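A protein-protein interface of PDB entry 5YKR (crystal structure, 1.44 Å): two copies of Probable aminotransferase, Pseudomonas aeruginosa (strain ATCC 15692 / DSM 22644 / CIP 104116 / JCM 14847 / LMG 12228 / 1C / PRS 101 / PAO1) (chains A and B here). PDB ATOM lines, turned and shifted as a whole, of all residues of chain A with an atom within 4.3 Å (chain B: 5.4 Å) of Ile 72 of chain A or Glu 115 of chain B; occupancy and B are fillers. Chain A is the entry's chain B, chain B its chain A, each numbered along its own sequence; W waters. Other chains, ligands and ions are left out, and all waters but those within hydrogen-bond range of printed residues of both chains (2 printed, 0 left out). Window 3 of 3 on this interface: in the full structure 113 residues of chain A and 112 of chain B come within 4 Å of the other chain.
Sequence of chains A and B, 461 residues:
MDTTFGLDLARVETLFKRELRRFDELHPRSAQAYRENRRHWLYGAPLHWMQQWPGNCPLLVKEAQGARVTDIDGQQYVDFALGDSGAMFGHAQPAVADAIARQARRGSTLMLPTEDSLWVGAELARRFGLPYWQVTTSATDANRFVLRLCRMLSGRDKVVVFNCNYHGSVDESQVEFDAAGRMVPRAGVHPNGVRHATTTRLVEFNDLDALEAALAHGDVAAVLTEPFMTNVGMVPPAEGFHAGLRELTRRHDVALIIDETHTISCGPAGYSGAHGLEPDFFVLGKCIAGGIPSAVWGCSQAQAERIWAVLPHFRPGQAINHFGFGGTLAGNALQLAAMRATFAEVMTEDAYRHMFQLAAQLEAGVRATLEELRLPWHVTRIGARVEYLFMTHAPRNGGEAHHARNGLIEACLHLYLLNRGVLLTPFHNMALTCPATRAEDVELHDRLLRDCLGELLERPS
The side-chain carboxylate (OE1) of Glu 115 of chain B is in salt-bridge range of the side-chain amino group (NZ) of Lys 62 of chain A. N of Val 61 of chain A lies within hydrogen-bond range of O of Pro 113 of chain B (3.0 Å).
The side-chain hydroxyl (OG1) of Thr 114 of chain B sits close to the backbone NH (N) of Asp 116 of chain B (3.3 Å). The guanidinium group (NH1) of Arg 29 of chain A lies within hydrogen-bond range of the backbone carbonyl oxygen (O) of Ile 72 of chain A (3.1 Å). The backbone NH of Ile 72 of chain A lies within hydrogen-bond range of the backbone carbonyl oxygen of Leu 60 of chain A, at 3.0 Å. The backbone carbonyl oxygen of Thr 114 of chain B lies within hydrogen-bond range of the side-chain hydroxyl of Ser 117 of chain B (2.7 Å). OG of Ser 30 of chain A is in hydrogen-bond range of N of Leu 60 of chain A, 2.9 Å away.
Among the printed residues, pairs that only touch across the chains: Leu 60 of chain A with Pro 113 of chain B, Leu 60 of chain A with Thr 114 of chain B, Leu 60 of chain A with Glu 115 of chain B, Leu 60 of chain A with Leu 118 of chain B, Val 61 of chain A with Thr 114 of chain B and Ile 72 of chain A with Glu 115 of chain B.
Printed residues of chain B within 4 Å of Leu 60 of chain A: Pro 113, Thr 114, Glu 115 and Leu 118. Printed residues of chain B within 4 Å of Val 61 of chain A: Pro 113 and Thr 114. Ile 72 of chain A touches just one residue of chain B: Glu 115 (3.8 Å). Printed residues of chain A within 4 Å of Pro 113 of chain B: Leu 60 (3.3 Å) and Val 61 (3.0 Å). Of the printed residues of chain A, Thr 114 of chain B touches Leu 60 (3.6 Å) and Val 61 (3.7 Å). Glu 115 of chain B touches just these residues of chain A: Leu 60 (3.9 Å), Lys 62 (3.6 Å) and Ile 72 (3.8 Å). Asp 116 of chain B touches none of the printed residues of chain A. The nearest printed residue of chain B that does not touch Ile 72 of chain A is Leu 118 of chain B (5.9 Å). The nearest printed residue of chain A that does not touch Glu 115 of chain B is Arg 29 of chain A (4.3 Å).
Of the 8 printed residues of chain B, 4 touch a printed residue of chain A. Hydrophobic or aromatic side chains of chain B that line the printed part of chain A: Pro 113 and Leu 118. Hydrophobic or aromatic side chains of chain A within 4 Å of the printed part of chain B: Leu 60 and Ile 72. Among the printed residues, 8 pairs touch across the chains.
No position is printed for both chains. Of the 8 pairs that touch across the chains among the printed residues, none has its exchanged pair printed and touching as well.
Water W1 lies within hydrogen-bond range of OE2 of Glu 115 of chain B (2.7 Å), NZ of Lys 62 of chain A (3.2 Å) and NH2 of Arg 29 of chain A (3.5 Å). Water W2 lies within hydrogen-bond range of the backbone carbonyl oxygen of Val 61 of chain A (2.7 Å) and the backbone NH of Glu 115 of chain B (2.8 Å).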
ATOM      1  N   ARG A  29      36.007 -23.704  19.689  1.00  0.00           N
ATOM      2  CA  ARG A  29      34.626 -24.091  19.857  1.00  0.00           C
ATOM      3  C   ARG A  29      33.832 -23.980  18.537  1.00  0.00           C
ATOM      4  O   ARG A  29      32.987 -24.848  18.239  1.00  0.00           O
ATOM      5  CB  ARG A  29      33.963 -23.330  20.979  1.00  0.00           C
ATOM      6  CG  ARG A  29      34.621 -23.602  22.354  1.00  0.00           C
ATOM      7  CD  ARG A  29      34.008 -22.796  23.453  1.00  0.00           C
ATOM      8  NE  ARG A  29      32.608 -23.137  23.637  1.00  0.00           N
ATOM      9  CZ  ARG A  29      31.798 -22.576  24.537  1.00  0.00           C
ATOM     10  NH1 ARG A  29      32.206 -21.616  25.369  1.00  0.00           N
ATOM     11  NH2 ARG A  29      30.533 -22.962  24.610  1.00  0.00           N
ATOM     12  N   SER A  30      34.081 -22.951  17.735  1.00  0.00           N
ATOM     13  CA  SER A  30      33.426 -22.882  16.414  1.00  0.00           C
ATOM     14  C   SER A  30      33.885 -24.041  15.540  1.00  0.00           C
ATOM     15  O   SER A  30      33.066 -24.612  14.791  1.00  0.00           O
ATOM     16  CB  SER A  30      33.646 -21.532  15.729  1.00  0.00           C
ATOM     17  OG  SER A  30      32.771 -20.571  16.293  1.00  0.00           O
ATOM     18  N   LEU A  60      30.457 -19.476  14.917  1.00  0.00           N
ATOM     19  CA  LEU A  60      29.130 -19.508  15.537  1.00  0.00           C
ATOM     20  C   LEU A  60      28.978 -18.291  16.457  1.00  0.00           C
ATOM     21  O   LEU A  60      29.841 -18.021  17.306  1.00  0.00           O
ATOM     22  CB  LEU A  60      28.815 -20.774  16.340  1.00  0.00           C
ATOM     23  CG  LEU A  60      28.117 -21.895  15.552  1.00  0.00           C
ATOM     24  CD1 LEU A  60      29.180 -22.455  14.596  1.00  0.00           C
ATOM     25  CD2 LEU A  60      27.580 -22.968  16.445  1.00  0.00           C
ATOM     26  N   VAL A  61      27.931 -17.532  16.199  1.00  0.00           N
ATOM     27  CA  VAL A  61      27.645 -16.323  16.966  1.00  0.00           C
ATOM     28  C   VAL A  61      26.887 -16.663  18.240  1.00  0.00           C
ATOM     29  O   VAL A  61      25.895 -17.373  18.192  1.00  0.00           O
ATOM     30  CB  VAL A  61      26.869 -15.323  16.115  1.00  0.00           C
ATOM     31  CG1 VAL A  61      26.436 -14.098  16.935  1.00  0.00           C
ATOM     32  CG2 VAL A  61      27.687 -14.949  14.888  1.00  0.00           C
ATOM     33  N   LYS A  62      27.328 -16.074  19.344  1.00  0.00           N
ATOM     34  CA  LYS A  62      26.592 -16.128  20.598  1.00  0.00           C
ATOM     35  C   LYS A  62      25.582 -14.996  20.729  1.00  0.00           C
ATOM     36  O   LYS A  62      24.403 -15.235  21.020  1.00  0.00           O
ATOM     37  CB  LYS A  62      27.573 -16.145  21.800  1.00  0.00           C
ATOM     38  CG  LYS A  62      26.882 -16.264  23.151  1.00  0.00           C
ATOM     39  CD  LYS A  62      26.289 -17.665  23.347  1.00  0.00           C
ATOM     40  CE  LYS A  62      25.738 -17.906  24.738  1.00  0.00           C
ATOM     41  NZ  LYS A  62      25.024 -19.213  24.737  1.00  0.00           N
ATOM     42  N   ASP A  71      31.361 -14.238  19.539  1.00  0.00           N
ATOM     43  CA  ASP A  71      31.246 -15.628  19.099  1.00  0.00           C
ATOM     44  C   ASP A  71      31.218 -16.615  20.288  1.00  0.00           C
ATOM     45  O   ASP A  71      31.357 -16.206  21.459  1.00  0.00           O
ATOM     46  CB  ASP A  71      32.285 -15.981  18.050  1.00  0.00           C
ATOM     47  CG  ASP A  71      33.710 -16.117  18.574  1.00  0.00           C
ATOM     48  OD1 ASP A  71      33.893 -16.214  19.816  1.00  0.00           O
ATOM     49  OD2 ASP A  71      34.640 -16.151  17.694  1.00  0.00           O
ATOM     50  N   ILE A  72      31.073 -17.897  20.009  1.00  0.00           N
ATOM     51  CA  ILE A  72      30.968 -18.876  21.085  1.00  0.00           C
ATOM     52  C   ILE A  72      32.292 -19.180  21.771  1.00  0.00           C
ATOM     53  O   ILE A  72      32.281 -19.837  22.799  1.00  0.00           O
ATOM     54  CB  ILE A  72      30.248 -20.162  20.623  1.00  0.00           C
ATOM     55  CG1 ILE A  72      31.010 -20.888  19.524  1.00  0.00           C
ATOM     56  CG2 ILE A  72      28.782 -19.877  20.196  1.00  0.00           C
ATOM     57  CD1 ILE A  72      30.464 -22.296  19.308  1.00  0.00           C
ATOM     58  N   ASP A  73      33.403 -18.716  21.211  1.00  0.00           N
ATOM     59  CA  ASP A  73      34.711 -18.730  21.847  1.00  0.00           C
ATOM     60  C   ASP A  73      34.973 -17.507  22.742  1.00  0.00           C
ATOM     61  O   ASP A  73      36.060 -17.371  23.282  1.00  0.00           O
ATOM     62  CB  ASP A  73      35.832 -18.910  20.815  1.00  0.00           C
ATOM     63  CG  ASP A  73      35.888 -20.321  20.259  1.00  0.00           C
ATOM     64  OD1 ASP A  73      36.381 -21.219  21.002  1.00  0.00           O
ATOM     65  OD2 ASP A  73      35.465 -20.526  19.103  1.00  0.00           O
ATOM     66  N   GLY A  74      34.003 -16.584  22.822  1.00  0.00           N
ATOM     67  CA  GLY A  74      34.196 -15.347  23.572  1.00  0.00           C
ATOM     68  C   GLY A  74      34.968 -14.253  22.891  1.00  0.00           C
ATOM     69  O   GLY A  74      35.260 -13.207  23.465  1.00  0.00           O
ATOM     70  N   PRO B 113      26.098 -19.020  11.359  1.00  0.00           N
ATOM     71  CA  PRO B 113      25.319 -19.914  12.184  1.00  0.00           C
ATOM     72  C   PRO B 113      25.364 -19.505  13.662  1.00  0.00           C
ATOM     73  O   PRO B 113      26.233 -18.735  14.105  1.00  0.00           O
ATOM     74  CB  PRO B 113      26.017 -21.277  11.970  1.00  0.00           C
ATOM     75  CG  PRO B 113      27.442 -20.906  11.774  1.00  0.00           C
ATOM     76  CD  PRO B 113      27.360 -19.635  10.950  1.00  0.00           C
ATOM     77  N   THR B 114      24.418 -20.049  14.416  1.00  0.00           N
ATOM     78  CA  THR B 114      24.346 -19.989  15.878  1.00  0.00           C
ATOM     79  C   THR B 114      24.224 -21.382  16.463  1.00  0.00           C
ATOM     80  O   THR B 114      24.117 -22.365  15.727  1.00  0.00           O
ATOM     81  CB  THR B 114      23.170 -19.148  16.345  1.00  0.00           C
ATOM     82  OG1 THR B 114      21.974 -19.839  15.956  1.00  0.00           O
ATOM     83  CG2 THR B 114      23.203 -17.739  15.737  1.00  0.00           C
ATOM     84  N   GLU B 115      24.211 -21.509  17.787  1.00  0.00           N
ATOM     85  CA  GLU B 115      24.052 -22.836  18.383  1.00  0.00           C
ATOM     86  C   GLU B 115      22.732 -23.502  18.011  1.00  0.00           C
ATOM     87  O   GLU B 115      22.648 -24.729  18.001  1.00  0.00           O
ATOM     88  CB  GLU B 115      24.222 -22.775  19.913  1.00  0.00           C
ATOM     89  CG  GLU B 115      25.659 -22.528  20.326  1.00  0.00           C
ATOM     90  CD  GLU B 115      25.844 -22.337  21.813  1.00  0.00           C
ATOM     91  OE1 GLU B 115      24.877 -22.061  22.543  1.00  0.00           O
ATOM     92  OE2 GLU B 115      26.973 -22.483  22.246  1.00  0.00           O
ATOM     93  N   ASP B 116      21.732 -22.716  17.626  1.00  0.00           N
ATOM     94  CA  ASP B 116      20.464 -23.332  17.238  1.00  0.00           C
ATOM     95  C   ASP B 116      20.631 -24.159  15.976  1.00  0.00           C
ATOM     96  O   ASP B 116      19.902 -25.122  15.764  1.00  0.00           O
ATOM     97  CB  ASP B 116      19.388 -22.287  17.015  1.00  0.00           C
ATOM     98  CG  ASP B 116      18.952 -21.567  18.294  1.00  0.00           C
ATOM     99  OD1 ASP B 116      19.063 -22.195  19.368  1.00  0.00           O
ATOM    100  OD2 ASP B 116      18.421 -20.424  18.202  1.00  0.00           O
ATOM    101  N   SER B 117      21.599 -23.819  15.119  1.00  0.00           N
ATOM    102  CA  SER B 117      21.830 -24.655  13.934  1.00  0.00           C
ATOM    103  C   SER B 117      22.281 -26.064  14.272  1.00  0.00           C
ATOM    104  O   SER B 117      21.930 -27.033  13.562  1.00  0.00           O
ATOM    105  CB  SER B 117      22.833 -24.011  12.976  1.00  0.00           C
ATOM    106  OG  SER B 117      24.148 -23.943  13.494  1.00  0.00           O
ATOM    107  N   LEU B 118      23.049 -26.191  15.350  1.00  0.00           N
ATOM    108  CA  LEU B 118      23.514 -27.515  15.779  1.00  0.00           C
ATOM    109  C   LEU B 118      22.286 -28.372  16.158  1.00  0.00           C
ATOM    110  O   LEU B 118      22.178 -29.519  15.695  1.00  0.00           O
ATOM    111  CB  LEU B 118      24.465 -27.390  16.974  1.00  0.00           C
ATOM    112  CG  LEU B 118      25.832 -26.847  16.682  1.00  0.00           C
ATOM    113  CD1 LEU B 118      26.449 -26.357  17.989  1.00  0.00           C
ATOM    114  CD2 LEU B 118      26.683 -27.915  16.067  1.00  0.00           C
ATOM    115  N   TRP B 119      21.392 -27.809  16.977  1.00  0.00           N
ATOM    116  CA  TRP B 119      20.263 -28.547  17.457  1.00  0.00           C
ATOM    117  C   TRP B 119      19.307 -28.913  16.324  1.00  0.00           C
ATOM    118  O   TRP B 119      18.840 -30.048  16.188  1.00  0.00           O
ATOM    119  CB  TRP B 119      19.583 -27.752  18.568  1.00  0.00           C
ATOM    120  CG  TRP B 119      18.509 -28.540  19.261  1.00  0.00           C
ATOM    121  CD1 TRP B 119      18.667 -29.206  20.439  1.00  0.00           C
ATOM    122  CD2 TRP B 119      17.165 -28.790  18.828  1.00  0.00           C
ATOM    123  NE1 TRP B 119      17.501 -29.848  20.753  1.00  0.00           N
ATOM    124  CE2 TRP B 119      16.553 -29.561  19.800  1.00  0.00           C
ATOM    125  CE3 TRP B 119      16.415 -28.380  17.740  1.00  0.00           C
ATOM    126  CZ2 TRP B 119      15.228 -30.022  19.676  1.00  0.00           C
ATOM    127  CZ3 TRP B 119      15.092 -28.793  17.647  1.00  0.00           C
ATOM    128  CH2 TRP B 119      14.515 -29.602  18.591  1.00  0.00           C
ATOM    129  N   ARG B 340      13.728 -24.146  15.959  1.00  0.00           N
ATOM    130  CA  ARG B 340      14.066 -24.939  17.120  1.00  0.00           C
ATOM    131  C   ARG B 340      12.867 -25.001  18.055  1.00  0.00           C
ATOM    132  O   ARG B 340      12.477 -26.084  18.514  1.00  0.00           O
ATOM    133  CB  ARG B 340      15.297 -24.408  17.816  1.00  0.00           C
ATOM    134  CG  ARG B 340      15.621 -25.120  19.115  1.00  0.00           C
ATOM    135  CD  ARG B 340      16.948 -24.702  19.620  1.00  0.00           C
ATOM    136  NE  ARG B 340      17.340 -25.470  20.798  1.00  0.00           N
ATOM    137  CZ  ARG B 340      18.549 -25.422  21.339  1.00  0.00           C
ATOM    138  NH1 ARG B 340      19.482 -24.583  20.850  1.00  0.00           N
ATOM    139  NH2 ARG B 340      18.816 -26.250  22.326  1.00  0.00           N
HETATM  140  O   HOH W   1      27.651 -21.048  24.377  1.00  0.00           O
HETATM  141  O   HOH W   2      24.704 -19.398  19.597  1.00  0.00           O
